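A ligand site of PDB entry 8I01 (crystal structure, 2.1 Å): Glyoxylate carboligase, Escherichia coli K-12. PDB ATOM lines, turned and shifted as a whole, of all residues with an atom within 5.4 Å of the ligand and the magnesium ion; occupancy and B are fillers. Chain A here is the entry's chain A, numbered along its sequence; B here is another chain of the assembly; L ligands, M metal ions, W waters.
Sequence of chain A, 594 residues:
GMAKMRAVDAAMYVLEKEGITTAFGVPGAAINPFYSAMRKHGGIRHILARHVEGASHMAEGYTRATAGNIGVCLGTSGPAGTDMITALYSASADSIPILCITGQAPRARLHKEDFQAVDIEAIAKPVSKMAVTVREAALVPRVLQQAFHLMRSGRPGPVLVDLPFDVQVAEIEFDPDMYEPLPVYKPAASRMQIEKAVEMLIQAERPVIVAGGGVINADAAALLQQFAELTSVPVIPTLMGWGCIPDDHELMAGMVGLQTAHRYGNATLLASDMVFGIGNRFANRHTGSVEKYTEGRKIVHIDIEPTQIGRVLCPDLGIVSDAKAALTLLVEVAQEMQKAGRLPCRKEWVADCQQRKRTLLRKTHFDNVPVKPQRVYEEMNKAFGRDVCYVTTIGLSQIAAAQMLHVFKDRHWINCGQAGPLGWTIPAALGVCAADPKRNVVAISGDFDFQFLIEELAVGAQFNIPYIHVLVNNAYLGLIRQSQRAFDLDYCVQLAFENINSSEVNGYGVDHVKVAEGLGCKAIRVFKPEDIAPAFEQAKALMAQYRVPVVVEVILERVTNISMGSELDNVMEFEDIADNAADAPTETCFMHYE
N of Asp 447 lies close to O3 of the ligand, at 3.2 Å. The backbone NH of Gly 478 lies within hydrogen-bond range of an oxygen (O7) of the ligand (3.2 Å). An oxygen (O7) of the ligand lies within hydrogen-bond range of the backbone NH of Leu 396, at 2.8 Å. N of Leu 479 sits at hydrogen-bond distance from O7 of the ligand (2.9 Å). O3 of the ligand sits close to N of Phe 448, at 2.9 Å. A nitrogen (N3) of the ligand is in hydrogen-bond range of the backbone carbonyl oxygen (O) of Gly 420 (2.9 Å). N of Ser 397 lies within hydrogen-bond range of O6 of the ligand (2.9 Å). O2 of the ligand lies within hydrogen-bond range of N of Asp 449, 3.0 Å away. The side-chain amide nitrogen (NE2) of Gln 116 of chain B lies close to a nitrogen (N3) of the ligand (3.4 Å).
The side-chain carboxylate (OD2) of Asp 447 sits close to the backbone NH (N) of Ala 475 (3.1 Å). OD1 of Asn 473 lies close to OD2 of Asp 447, at 3.2 Å. The backbone carbonyl oxygen of Gly 420 sits at hydrogen-bond distance from the side-chain amide nitrogen of Gln 116 of chain B (3.5 Å). OG of Ser 397 sits at hydrogen-bond distance from N of Gly 446 (3.3 Å). OG of Ser 445 sits at hydrogen-bond distance from OD2 of Asp 449 (2.6 Å). NE2 of Gln 116 of chain B sits at hydrogen-bond distance from O of Ala 419 (2.8 Å).
CD1 of Ile 394 touches C7 of the ligand, at 3.8 Å. CA of Gly 395 touches O7 of the ligand, at 3.5 Å. Leu 422 touches the ligand. Gly 446 touches the ligand (CA to O2, 3.5 Å). CE2 of Phe 452 touches C2 of the ligand, at 3.8 Å. Leu 477 touches the ligand. Ile 480 touches the ligand. CG1 of Val 26 of chain B touches C10 of the ligand, 3.9 Å away. Pro 27 of chain B touches the ligand (O to C10, 3.3 Å). Val 52 of chain B touches the ligand (CG2 to N1, 3.6 Å). CG2 of Thr 76 of chain B touches C5 of the ligand (3.7 Å). CG of Pro 79 of chain B touches N2 of the ligand, at 3.7 Å. Ala 80 of chain B touches the ligand (N to C2, 3.9 Å). Asp 83 of chain B touches the ligand. Hydrophobic or aromatic side chains that line the ligand: Ile 394, Leu 396, Leu 422, Phe 448, Phe 452, Leu 477, Leu 479, Ile 480, Val 26 of chain B, Val 52 of chain B and Pro 79 of chain B. Of the 34 residues printed, 25 come within 4 Å of the ligand.
Three residues have an atom within 4 Å of the magnesium ion: Asp 447, Asn 474 and Tyr 476. The nearest printed residue that does not touch the magnesium ion is Gly 478 (4.02 Å).
The side-chain amide oxygen (OD1) of Asn 474 binds the magnesium ion (2.0 Å). The magnesium ion is bound by the backbone carbonyl oxygen (O) of Tyr 476, at 2.1 Å. O3 of the ligand is bound to the magnesium ion. The side-chain carboxylate (OD1) of Asp 447 binds the magnesium ion, 2.2 Å away. O5 of the ligand is bound to the magnesium ion. Water W4 is bound to the magnesium ion, 2.5 Å away. The magnesium ion has six donor atoms within binding distance.
Water W4 lies within hydrogen-bond range of O of Val 472, O6 of the ligand, ND2 of Asn 474 and N of Asp 447. Water W1 lies within hydrogen-bond range of O2 of the ligand (2.7 Å), N of Gly 446 (2.7 Å), OG of Ser 397 (2.7 Å) and O of Ile 394 (2.8 Å). Water W2 lies within hydrogen-bond range of O of Val 26 of chain B (2.7 Å), N of Thr 76 of chain B (3.0 Å) and N1 of the ligand (3.1 Å). Water W3 lies within hydrogen-bond range of OE1 of Gln 116 of chain B and N3 of the ligand.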
ATOM      1  N   ILE A 394     -13.277 -27.811  -4.852  1.00  0.00           N
ATOM      2  CA  ILE A 394     -13.396 -26.360  -4.893  1.00  0.00           C
ATOM      3  C   ILE A 394     -12.997 -25.883  -6.273  1.00  0.00           C
ATOM      4  O   ILE A 394     -12.186 -26.530  -6.947  1.00  0.00           O
ATOM      5  CB  ILE A 394     -12.506 -25.695  -3.799  1.00  0.00           C
ATOM      6  CG1 ILE A 394     -12.777 -24.186  -3.689  1.00  0.00           C
ATOM      7  CG2 ILE A 394     -11.058 -25.957  -4.114  1.00  0.00           C
ATOM      8  CD1 ILE A 394     -12.141 -23.572  -2.450  1.00  0.00           C
ATOM      9  N   GLY A 395     -13.492 -24.715  -6.657  1.00  0.00           N
ATOM     10  CA  GLY A 395     -13.293 -24.142  -7.975  1.00  0.00           C
ATOM     11  C   GLY A 395     -14.626 -23.788  -8.610  1.00  0.00           C
ATOM     12  O   GLY A 395     -15.691 -24.135  -8.113  1.00  0.00           O
ATOM     13  N   LEU A 396     -14.535 -23.103  -9.758  1.00  0.00           N
ATOM     14  CA  LEU A 396     -15.756 -22.908 -10.539  1.00  0.00           C
ATOM     15  C   LEU A 396     -16.347 -24.257 -10.957  1.00  0.00           C
ATOM     16  O   LEU A 396     -17.584 -24.418 -11.016  1.00  0.00           O
ATOM     17  CB  LEU A 396     -15.463 -22.054 -11.770  1.00  0.00           C
ATOM     18  CG  LEU A 396     -15.075 -20.603 -11.433  1.00  0.00           C
ATOM     19  CD1 LEU A 396     -14.939 -19.770 -12.717  1.00  0.00           C
ATOM     20  CD2 LEU A 396     -16.089 -19.981 -10.481  1.00  0.00           C
ATOM     21  N   SER A 397     -15.499 -25.248 -11.199  1.00  0.00           N
ATOM     22  CA  SER A 397     -15.970 -26.593 -11.461  1.00  0.00           C
ATOM     23  C   SER A 397     -16.925 -27.058 -10.365  1.00  0.00           C
ATOM     24  O   SER A 397     -18.014 -27.591 -10.643  1.00  0.00           O
ATOM     25  CB  SER A 397     -14.763 -27.523 -11.506  1.00  0.00           C
ATOM     26  OG  SER A 397     -14.038 -27.359 -10.277  1.00  0.00           O
ATOM     27  N   ALA A 419     -12.719 -26.426   4.443  1.00  0.00           N
ATOM     28  CA  ALA A 419     -11.297 -26.219   4.171  1.00  0.00           C
ATOM     29  C   ALA A 419     -10.941 -26.202   2.686  1.00  0.00           C
ATOM     30  O   ALA A 419     -10.004 -25.496   2.307  1.00  0.00           O
ATOM     31  CB  ALA A 419     -10.454 -27.297   4.862  1.00  0.00           C
ATOM     32  N   GLY A 420     -11.641 -26.979   1.843  1.00  0.00           N
ATOM     33  CA  GLY A 420     -11.433 -26.905   0.405  1.00  0.00           C
ATOM     34  C   GLY A 420     -10.003 -27.051  -0.117  1.00  0.00           C
ATOM     35  O   GLY A 420      -9.571 -26.269  -0.960  1.00  0.00           O
ATOM     36  N   PRO A 421      -9.239 -28.040   0.347  1.00  0.00           N
ATOM     37  CA  PRO A 421      -7.853 -28.191  -0.143  1.00  0.00           C
ATOM     38  C   PRO A 421      -7.787 -28.754  -1.556  1.00  0.00           C
ATOM     39  O   PRO A 421      -8.293 -29.851  -1.817  1.00  0.00           O
ATOM     40  CB  PRO A 421      -7.230 -29.179   0.861  1.00  0.00           C
ATOM     41  CG  PRO A 421      -8.354 -29.954   1.384  1.00  0.00           C
ATOM     42  CD  PRO A 421      -9.570 -29.062   1.352  1.00  0.00           C
ATOM     43  N   LEU A 422      -7.102 -28.035  -2.443  1.00  0.00           N
ATOM     44  CA  LEU A 422      -6.908 -28.532  -3.797  1.00  0.00           C
ATOM     45  C   LEU A 422      -6.155 -29.856  -3.769  1.00  0.00           C
ATOM     46  O   LEU A 422      -5.295 -30.075  -2.913  1.00  0.00           O
ATOM     47  CB  LEU A 422      -6.159 -27.505  -4.645  1.00  0.00           C
ATOM     48  CG  LEU A 422      -6.955 -26.271  -5.084  1.00  0.00           C
ATOM     49  CD1 LEU A 422      -5.995 -25.176  -5.617  1.00  0.00           C
ATOM     50  CD2 LEU A 422      -8.042 -26.612  -6.160  1.00  0.00           C
ATOM     51  N   SER A 445     -13.569 -32.318 -11.032  1.00  0.00           N
ATOM     52  CA  SER A 445     -12.398 -31.472 -10.798  1.00  0.00           C
ATOM     53  C   SER A 445     -12.240 -30.468 -11.926  1.00  0.00           C
ATOM     54  O   SER A 445     -12.461 -30.799 -13.100  1.00  0.00           O
ATOM     55  CB  SER A 445     -11.056 -32.234 -10.775  1.00  0.00           C
ATOM     56  OG  SER A 445     -10.902 -32.977  -9.591  1.00  0.00           O
ATOM     57  N   GLY A 446     -11.750 -29.281 -11.577  1.00  0.00           N
ATOM     58  CA  GLY A 446     -11.089 -28.440 -12.554  1.00  0.00           C
ATOM     59  C   GLY A 446      -9.675 -28.943 -12.811  1.00  0.00           C
ATOM     60  O   GLY A 446      -9.177 -29.851 -12.137  1.00  0.00           O
ATOM     61  N   ASP A 447      -9.031 -28.344 -13.829  1.00  0.00           N
ATOM     62  CA  ASP A 447      -7.700 -28.843 -14.208  1.00  0.00           C
ATOM     63  C   ASP A 447      -6.661 -28.631 -13.101  1.00  0.00           C
ATOM     64  O   ASP A 447      -5.813 -29.503 -12.890  1.00  0.00           O
ATOM     65  CB  ASP A 447      -7.221 -28.233 -15.538  1.00  0.00           C
ATOM     66  CG  ASP A 447      -7.492 -26.732 -15.658  1.00  0.00           C
ATOM     67  OD1 ASP A 447      -8.582 -26.242 -15.305  1.00  0.00           O
ATOM     68  OD2 ASP A 447      -6.584 -26.033 -16.177  1.00  0.00           O
ATOM     69  N   PHE A 448      -6.729 -27.520 -12.366  1.00  0.00           N
ATOM     70  CA  PHE A 448      -5.696 -27.237 -11.375  1.00  0.00           C
ATOM     71  C   PHE A 448      -5.812 -28.184 -10.171  1.00  0.00           C
ATOM     72  O   PHE A 448      -4.823 -28.763  -9.733  1.00  0.00           O
ATOM     73  CB  PHE A 448      -5.791 -25.773 -10.955  1.00  0.00           C
ATOM     74  CG  PHE A 448      -4.587 -25.220 -10.218  1.00  0.00           C
ATOM     75  CD1 PHE A 448      -3.309 -25.267 -10.768  1.00  0.00           C
ATOM     76  CD2 PHE A 448      -4.752 -24.578  -8.999  1.00  0.00           C
ATOM     77  CE1 PHE A 448      -2.201 -24.718 -10.090  1.00  0.00           C
ATOM     78  CE2 PHE A 448      -3.671 -24.040  -8.317  1.00  0.00           C
ATOM     79  CZ  PHE A 448      -2.385 -24.108  -8.867  1.00  0.00           C
ATOM     80  N   ASP A 449      -7.030 -28.374  -9.663  1.00  0.00           N
ATOM     81  CA  ASP A 449      -7.275 -29.378  -8.611  1.00  0.00           C
ATOM     82  C   ASP A 449      -6.815 -30.751  -9.063  1.00  0.00           C
ATOM     83  O   ASP A 449      -6.229 -31.509  -8.270  1.00  0.00           O
ATOM     84  CB  ASP A 449      -8.787 -29.400  -8.270  1.00  0.00           C
ATOM     85  CG  ASP A 449      -9.226 -30.611  -7.430  1.00  0.00           C
ATOM     86  OD1 ASP A 449      -8.587 -30.960  -6.409  1.00  0.00           O
ATOM     87  OD2 ASP A 449     -10.272 -31.204  -7.747  1.00  0.00           O
ATOM     88  N   PHE A 450      -7.047 -31.082 -10.327  1.00  0.00           N
ATOM     89  CA  PHE A 450      -6.709 -32.411 -10.840  1.00  0.00           C
ATOM     90  C   PHE A 450      -5.204 -32.630 -10.831  1.00  0.00           C
ATOM     91  O   PHE A 450      -4.742 -33.752 -10.599  1.00  0.00           O
ATOM     92  CB  PHE A 450      -7.286 -32.547 -12.258  1.00  0.00           C
ATOM     93  CG  PHE A 450      -7.255 -33.945 -12.807  1.00  0.00           C
ATOM     94  CD1 PHE A 450      -8.090 -34.920 -12.309  1.00  0.00           C
ATOM     95  CD2 PHE A 450      -6.409 -34.275 -13.828  1.00  0.00           C
ATOM     96  CE1 PHE A 450      -8.071 -36.196 -12.820  1.00  0.00           C
ATOM     97  CE2 PHE A 450      -6.397 -35.549 -14.354  1.00  0.00           C
ATOM     98  CZ  PHE A 450      -7.227 -36.512 -13.838  1.00  0.00           C
ATOM     99  N   PHE A 452      -2.811 -31.271  -8.697  1.00  0.00           N
ATOM    100  CA  PHE A 452      -2.108 -31.274  -7.408  1.00  0.00           C
ATOM    101  C   PHE A 452      -1.651 -32.670  -7.003  1.00  0.00           C
ATOM    102  O   PHE A 452      -0.490 -32.883  -6.636  1.00  0.00           O
ATOM    103  CB  PHE A 452      -3.020 -30.725  -6.294  1.00  0.00           C
ATOM    104  CG  PHE A 452      -2.799 -29.247  -5.931  1.00  0.00           C
ATOM    105  CD1 PHE A 452      -2.918 -28.245  -6.878  1.00  0.00           C
ATOM    106  CD2 PHE A 452      -2.564 -28.872  -4.592  1.00  0.00           C
ATOM    107  CE1 PHE A 452      -2.741 -26.899  -6.542  1.00  0.00           C
ATOM    108  CE2 PHE A 452      -2.409 -27.526  -4.234  1.00  0.00           C
ATOM    109  CZ  PHE A 452      -2.491 -26.542  -5.212  1.00  0.00           C
ATOM    110  N   VAL A 472     -13.007 -30.832 -16.021  1.00  0.00           N
ATOM    111  CA  VAL A 472     -13.433 -29.708 -16.855  1.00  0.00           C
ATOM    112  C   VAL A 472     -12.251 -28.743 -16.942  1.00  0.00           C
ATOM    113  O   VAL A 472     -11.828 -28.154 -15.935  1.00  0.00           O
ATOM    114  CB  VAL A 472     -14.727 -29.056 -16.327  1.00  0.00           C
ATOM    115  CG1 VAL A 472     -15.852 -30.073 -16.341  1.00  0.00           C
ATOM    116  CG2 VAL A 472     -14.580 -28.505 -14.909  1.00  0.00           C
ATOM    117  N   ASN A 473     -11.690 -28.596 -18.135  1.00  0.00           N
ATOM    118  CA  ASN A 473     -10.374 -27.992 -18.326  1.00  0.00           C
ATOM    119  C   ASN A 473     -10.540 -26.641 -19.000  1.00  0.00           C
ATOM    120  O   ASN A 473     -10.869 -26.569 -20.199  1.00  0.00           O
ATOM    121  CB  ASN A 473      -9.479 -28.919 -19.147  1.00  0.00           C
ATOM    122  CG  ASN A 473      -8.079 -28.350 -19.392  1.00  0.00           C
ATOM    123  OD1 ASN A 473      -7.706 -27.319 -18.844  1.00  0.00           O
ATOM    124  ND2 ASN A 473      -7.297 -29.048 -20.205  1.00  0.00           N
ATOM    125  N   ASN A 474     -10.299 -25.558 -18.254  1.00  0.00           N
ATOM    126  CA  ASN A 474     -10.263 -24.225 -18.824  1.00  0.00           C
ATOM    127  C   ASN A 474      -8.848 -23.656 -18.903  1.00  0.00           C
ATOM    128  O   ASN A 474      -8.674 -22.493 -19.269  1.00  0.00           O
ATOM    129  CB  ASN A 474     -11.198 -23.282 -18.046  1.00  0.00           C
ATOM    130  CG  ASN A 474     -10.914 -23.259 -16.536  1.00  0.00           C
ATOM    131  OD1 ASN A 474      -9.839 -23.634 -16.074  1.00  0.00           O
ATOM    132  ND2 ASN A 474     -11.900 -22.808 -15.769  1.00  0.00           N
ATOM    133  N   ALA A 475      -7.829 -24.452 -18.569  1.00  0.00           N
ATOM    134  CA  ALA A 475      -6.438 -23.977 -18.509  1.00  0.00           C
ATOM    135  C   ALA A 475      -6.320 -22.681 -17.683  1.00  0.00           C
ATOM    136  O   ALA A 475      -5.521 -21.783 -17.996  1.00  0.00           O
ATOM    137  CB  ALA A 475      -5.846 -23.796 -19.903  1.00  0.00           C
ATOM    138  N   TYR A 476      -7.088 -22.605 -16.600  1.00  0.00           N
ATOM    139  CA  TYR A 476      -7.113 -21.452 -15.708  1.00  0.00           C
ATOM    140  C   TYR A 476      -7.304 -21.929 -14.274  1.00  0.00           C
ATOM    141  O   TYR A 476      -7.893 -22.993 -14.036  1.00  0.00           O
ATOM    142  CB  TYR A 476      -8.298 -20.530 -16.036  1.00  0.00           C
ATOM    143  CG  TYR A 476      -8.040 -19.209 -16.751  1.00  0.00           C
ATOM    144  CD1 TYR A 476      -7.554 -18.100 -16.066  1.00  0.00           C
ATOM    145  CD2 TYR A 476      -8.391 -19.043 -18.081  1.00  0.00           C
ATOM    146  CE1 TYR A 476      -7.380 -16.886 -16.705  1.00  0.00           C
ATOM    147  CE2 TYR A 476      -8.223 -17.827 -18.736  1.00  0.00           C
ATOM    148  CZ  TYR A 476      -7.719 -16.754 -18.038  1.00  0.00           C
ATOM    149  OH  TYR A 476      -7.550 -15.547 -18.682  1.00  0.00           O
ATOM    150  N   LEU A 477      -6.841 -21.131 -13.305  1.00  0.00           N
ATOM    151  CA  LEU A 477      -7.399 -21.170 -11.947  1.00  0.00           C
ATOM    152  C   LEU A 477      -8.673 -20.324 -11.978  1.00  0.00           C
ATOM    153  O   LEU A 477      -8.657 -19.123 -11.696  1.00  0.00           O
ATOM    154  CB  LEU A 477      -6.449 -20.635 -10.889  1.00  0.00           C
ATOM    155  CG  LEU A 477      -4.948 -20.880 -10.819  1.00  0.00           C
ATOM    156  CD1 LEU A 477      -4.371 -20.676  -9.417  1.00  0.00           C
ATOM    157  CD2 LEU A 477      -4.554 -22.180 -11.409  1.00  0.00           C
ATOM    158  N   GLY A 478      -9.772 -20.949 -12.396  1.00  0.00           N
ATOM    159  CA  GLY A 478     -10.913 -20.158 -12.842  1.00  0.00           C
ATOM    160  C   GLY A 478     -11.555 -19.351 -11.721  1.00  0.00           C
ATOM    161  O   GLY A 478     -11.910 -18.191 -11.915  1.00  0.00           O
ATOM    162  N   LEU A 479     -11.659 -19.944 -10.531  1.00  0.00           N
ATOM    163  CA  LEU A 479     -12.272 -19.217  -9.428  1.00  0.00           C
ATOM    164  C   LEU A 479     -11.437 -18.014  -9.046  1.00  0.00           C
ATOM    165  O   LEU A 479     -11.989 -16.954  -8.738  1.00  0.00           O
ATOM    166  CB  LEU A 479     -12.467 -20.141  -8.217  1.00  0.00           C
ATOM    167  CG  LEU A 479     -13.032 -19.506  -6.929  1.00  0.00           C
ATOM    168  CD1 LEU A 479     -14.368 -18.813  -7.160  1.00  0.00           C
ATOM    169  CD2 LEU A 479     -13.189 -20.568  -5.841  1.00  0.00           C
ATOM    170  N   ILE A 480     -10.107 -18.124  -9.137  1.00  0.00           N
ATOM    171  CA  ILE A 480      -9.241 -17.004  -8.748  1.00  0.00           C
ATOM    172  C   ILE A 480      -9.287 -15.906  -9.805  1.00  0.00           C
ATOM    173  O   ILE A 480      -9.280 -14.714  -9.482  1.00  0.00           O
ATOM    174  CB  ILE A 480      -7.799 -17.473  -8.499  1.00  0.00           C
ATOM    175  CG1 ILE A 480      -7.806 -18.751  -7.656  1.00  0.00           C
ATOM    176  CG2 ILE A 480      -6.996 -16.374  -7.817  1.00  0.00           C
ATOM    177  CD1 ILE A 480      -8.644 -18.674  -6.364  1.00  0.00           C
ATOM    178  N   LEU A 495      -2.763 -21.429 -16.843  1.00  0.00           N
ATOM    179  CA  LEU A 495      -1.994 -22.667 -16.914  1.00  0.00           C
ATOM    180  C   LEU A 495      -1.622 -23.064 -18.348  1.00  0.00           C
ATOM    181  O   LEU A 495      -0.937 -24.074 -18.538  1.00  0.00           O
ATOM    182  CB  LEU A 495      -2.795 -23.799 -16.247  1.00  0.00           C
ATOM    183  CG  LEU A 495      -3.104 -23.561 -14.770  1.00  0.00           C
ATOM    184  CD1 LEU A 495      -4.071 -24.614 -14.229  1.00  0.00           C
ATOM    185  CD2 LEU A 495      -1.781 -23.572 -13.950  1.00  0.00           C
ATOM    186  N   VAL B  26       0.870 -19.767  -5.338  1.00  0.00           N
ATOM    187  CA  VAL B  26      -0.443 -20.150  -5.829  1.00  0.00           C
ATOM    188  C   VAL B  26      -1.411 -19.112  -5.273  1.00  0.00           C
ATOM    189  O   VAL B  26      -1.627 -19.065  -4.058  1.00  0.00           O
ATOM    190  CB  VAL B  26      -0.841 -21.565  -5.381  1.00  0.00           C
ATOM    191  CG1 VAL B  26      -2.314 -21.864  -5.789  1.00  0.00           C
ATOM    192  CG2 VAL B  26       0.118 -22.592  -5.962  1.00  0.00           C
ATOM    193  N   PRO B  27      -1.964 -18.241  -6.099  1.00  0.00           N
ATOM    194  CA  PRO B  27      -2.864 -17.207  -5.588  1.00  0.00           C
ATOM    195  C   PRO B  27      -4.204 -17.804  -5.182  1.00  0.00           C
ATOM    196  O   PRO B  27      -4.525 -18.969  -5.470  1.00  0.00           O
ATOM    197  CB  PRO B  27      -3.002 -16.237  -6.771  1.00  0.00           C
ATOM    198  CG  PRO B  27      -2.834 -17.104  -7.954  1.00  0.00           C
ATOM    199  CD  PRO B  27      -1.868 -18.208  -7.569  1.00  0.00           C
ATOM    200  N   GLY B  28      -4.954 -17.003  -4.428  1.00  0.00           N
ATOM    201  CA  GLY B  28      -6.310 -17.304  -3.986  1.00  0.00           C
ATOM    202  C   GLY B  28      -6.925 -16.010  -3.507  1.00  0.00           C
ATOM    203  O   GLY B  28      -6.238 -14.988  -3.361  1.00  0.00           O
ATOM    204  N   VAL B  52       0.773 -26.234  -3.718  1.00  0.00           N
ATOM    205  CA  VAL B  52       1.386 -25.290  -2.786  1.00  0.00           C
ATOM    206  C   VAL B  52       2.650 -25.876  -2.173  1.00  0.00           C
ATOM    207  O   VAL B  52       3.618 -25.155  -1.940  1.00  0.00           O
ATOM    208  CB  VAL B  52       0.374 -24.859  -1.705  1.00  0.00           C
ATOM    209  CG1 VAL B  52       1.084 -24.177  -0.535  1.00  0.00           C
ATOM    210  CG2 VAL B  52      -0.663 -23.932  -2.327  1.00  0.00           C
ATOM    211  N   THR B  76      -2.713 -18.651  -0.288  1.00  0.00           N
ATOM    212  CA  THR B  76      -3.932 -18.088   0.271  1.00  0.00           C
ATOM    213  C   THR B  76      -4.110 -18.608   1.713  1.00  0.00           C
ATOM    214  O   THR B  76      -3.177 -19.146   2.308  1.00  0.00           O
ATOM    215  CB  THR B  76      -5.132 -18.398  -0.636  1.00  0.00           C
ATOM    216  OG1 THR B  76      -6.253 -17.593  -0.237  1.00  0.00           O
ATOM    217  CG2 THR B  76      -5.554 -19.895  -0.549  1.00  0.00           C
ATOM    218  N   PRO B  79      -5.959 -24.128   3.737  1.00  0.00           N
ATOM    219  CA  PRO B  79      -5.120 -25.279   3.373  1.00  0.00           C
ATOM    220  C   PRO B  79      -3.810 -24.918   2.691  1.00  0.00           C
ATOM    221  O   PRO B  79      -2.921 -25.774   2.619  1.00  0.00           O
ATOM    222  CB  PRO B  79      -6.019 -26.090   2.437  1.00  0.00           C
ATOM    223  CG  PRO B  79      -6.809 -25.038   1.770  1.00  0.00           C
ATOM    224  CD  PRO B  79      -7.163 -24.058   2.897  1.00  0.00           C
ATOM    225  N   ALA B  80      -3.676 -23.727   2.106  1.00  0.00           N
ATOM    226  CA  ALA B  80      -2.388 -23.324   1.567  1.00  0.00           C
ATOM    227  C   ALA B  80      -1.340 -23.240   2.667  1.00  0.00           C
ATOM    228  O   ALA B  80      -0.242 -23.782   2.520  1.00  0.00           O
ATOM    229  CB  ALA B  80      -2.502 -21.989   0.823  1.00  0.00           C
ATOM    230  N   ASP B  83      -0.358 -26.630   3.822  1.00  0.00           N
ATOM    231  CA  ASP B  83       0.487 -27.274   2.809  1.00  0.00           C
ATOM    232  C   ASP B  83       1.930 -26.776   2.823  1.00  0.00           C
ATOM    233  O   ASP B  83       2.768 -27.347   2.114  1.00  0.00           O
ATOM    234  CB  ASP B  83      -0.086 -27.026   1.403  1.00  0.00           C
ATOM    235  CG  ASP B  83      -1.246 -27.988   1.024  1.00  0.00           C
ATOM    236  OD1 ASP B  83      -1.560 -28.957   1.754  1.00  0.00           O
ATOM    237  OD2 ASP B  83      -1.829 -27.751  -0.055  1.00  0.00           O
ATOM    238  N   GLN B 116     -12.255 -21.291   5.318  1.00  0.00           N
ATOM    239  CA  GLN B 116     -10.806 -21.460   5.174  1.00  0.00           C
ATOM    240  C   GLN B 116     -10.002 -20.598   6.151  1.00  0.00           C
ATOM    241  O   GLN B 116      -8.867 -20.245   5.878  1.00  0.00           O
ATOM    242  CB  GLN B 116     -10.352 -21.169   3.740  1.00  0.00           C
ATOM    243  CG  GLN B 116     -10.682 -22.314   2.791  1.00  0.00           C
ATOM    244  CD  GLN B 116     -10.097 -22.126   1.395  1.00  0.00           C
ATOM    245  OE1 GLN B 116      -9.826 -21.003   0.969  1.00  0.00           O
ATOM    246  NE2 GLN B 116      -9.898 -23.242   0.678  1.00  0.00           N
HETATM  247  N1  LIG L   1      -4.246 -23.470  -2.550  1.00  0.00           N
HETATM  248  C1  LIG L   1      -4.847 -24.517  -1.943  1.00  0.00           C
HETATM  249  C2  LIG L   1      -3.972 -25.561  -1.331  1.00  0.00           C
HETATM  250  N2  LIG L   1      -6.171 -24.689  -1.818  1.00  0.00           N
HETATM  251  C3  LIG L   1      -6.977 -23.752  -2.345  1.00  0.00           C
HETATM  252  N3  LIG L   1      -8.297 -23.942  -2.199  1.00  0.00           N
HETATM  253  C4  LIG L   1      -6.440 -22.625  -3.042  1.00  0.00           C
HETATM  254  C5  LIG L   1      -5.066 -22.550  -3.080  1.00  0.00           C
HETATM  255  C6  LIG L   1      -7.289 -21.516  -3.632  1.00  0.00           C
HETATM  256  N4  LIG L   1      -8.098 -21.944  -4.803  1.00  0.00           N
HETATM  257  C7  LIG L   1      -9.384 -22.255  -4.718  1.00  0.00           C
HETATM  258  S1  LIG L   1     -10.036 -22.678  -6.214  1.00  0.00           S
HETATM  259  C8  LIG L   1      -8.525 -22.399  -7.001  1.00  0.00           C
HETATM  260  C9  LIG L   1      -7.577 -22.011  -6.092  1.00  0.00           C
HETATM  261  C10 LIG L   1      -6.145 -21.687  -6.362  1.00  0.00           C
HETATM  262  C11 LIG L   1      -8.368 -22.637  -8.485  1.00  0.00           C
HETATM  263  C12 LIG L   1      -8.944 -23.969  -8.902  1.00  0.00           C
HETATM  264  O1  LIG L   1      -8.806 -24.147 -10.333  1.00  0.00           O
HETATM  265  P1  LIG L   1      -9.372 -25.404 -11.107  1.00  0.00           P
HETATM  266  O2  LIG L   1      -9.319 -26.582 -10.165  1.00  0.00           O
HETATM  267  O3  LIG L   1      -8.798 -25.471 -12.472  1.00  0.00           O
HETATM  268  O4  LIG L   1     -10.876 -24.944 -11.240  1.00  0.00           O
HETATM  269  P2  LIG L   1     -11.691 -23.809 -11.982  1.00  0.00           P
HETATM  270  O5  LIG L   1     -10.857 -23.257 -13.102  1.00  0.00           O
HETATM  271  O6  LIG L   1     -12.963 -24.517 -12.491  1.00  0.00           O
HETATM  272  O7  LIG L   1     -11.986 -22.773 -10.913  1.00  0.00           O
HETATM  273 MG    MG M   1      -9.383 -24.481 -14.280  1.00  0.00          MG
HETATM  274  O   HOH W   1     -11.527 -27.801  -9.351  1.00  0.00           O
HETATM  275  O   HOH W   2      -2.463 -20.911  -2.277  1.00  0.00           O
HETATM  276  O   HOH W   3      -9.942 -21.071  -1.569  1.00  0.00           O
HETATM  277  O   HOH W   4     -11.369 -25.876 -14.642  1.00  0.00           O
HETATM  278  O   HOH W   5     -14.850 -24.414 -14.683  1.00  0.00           O
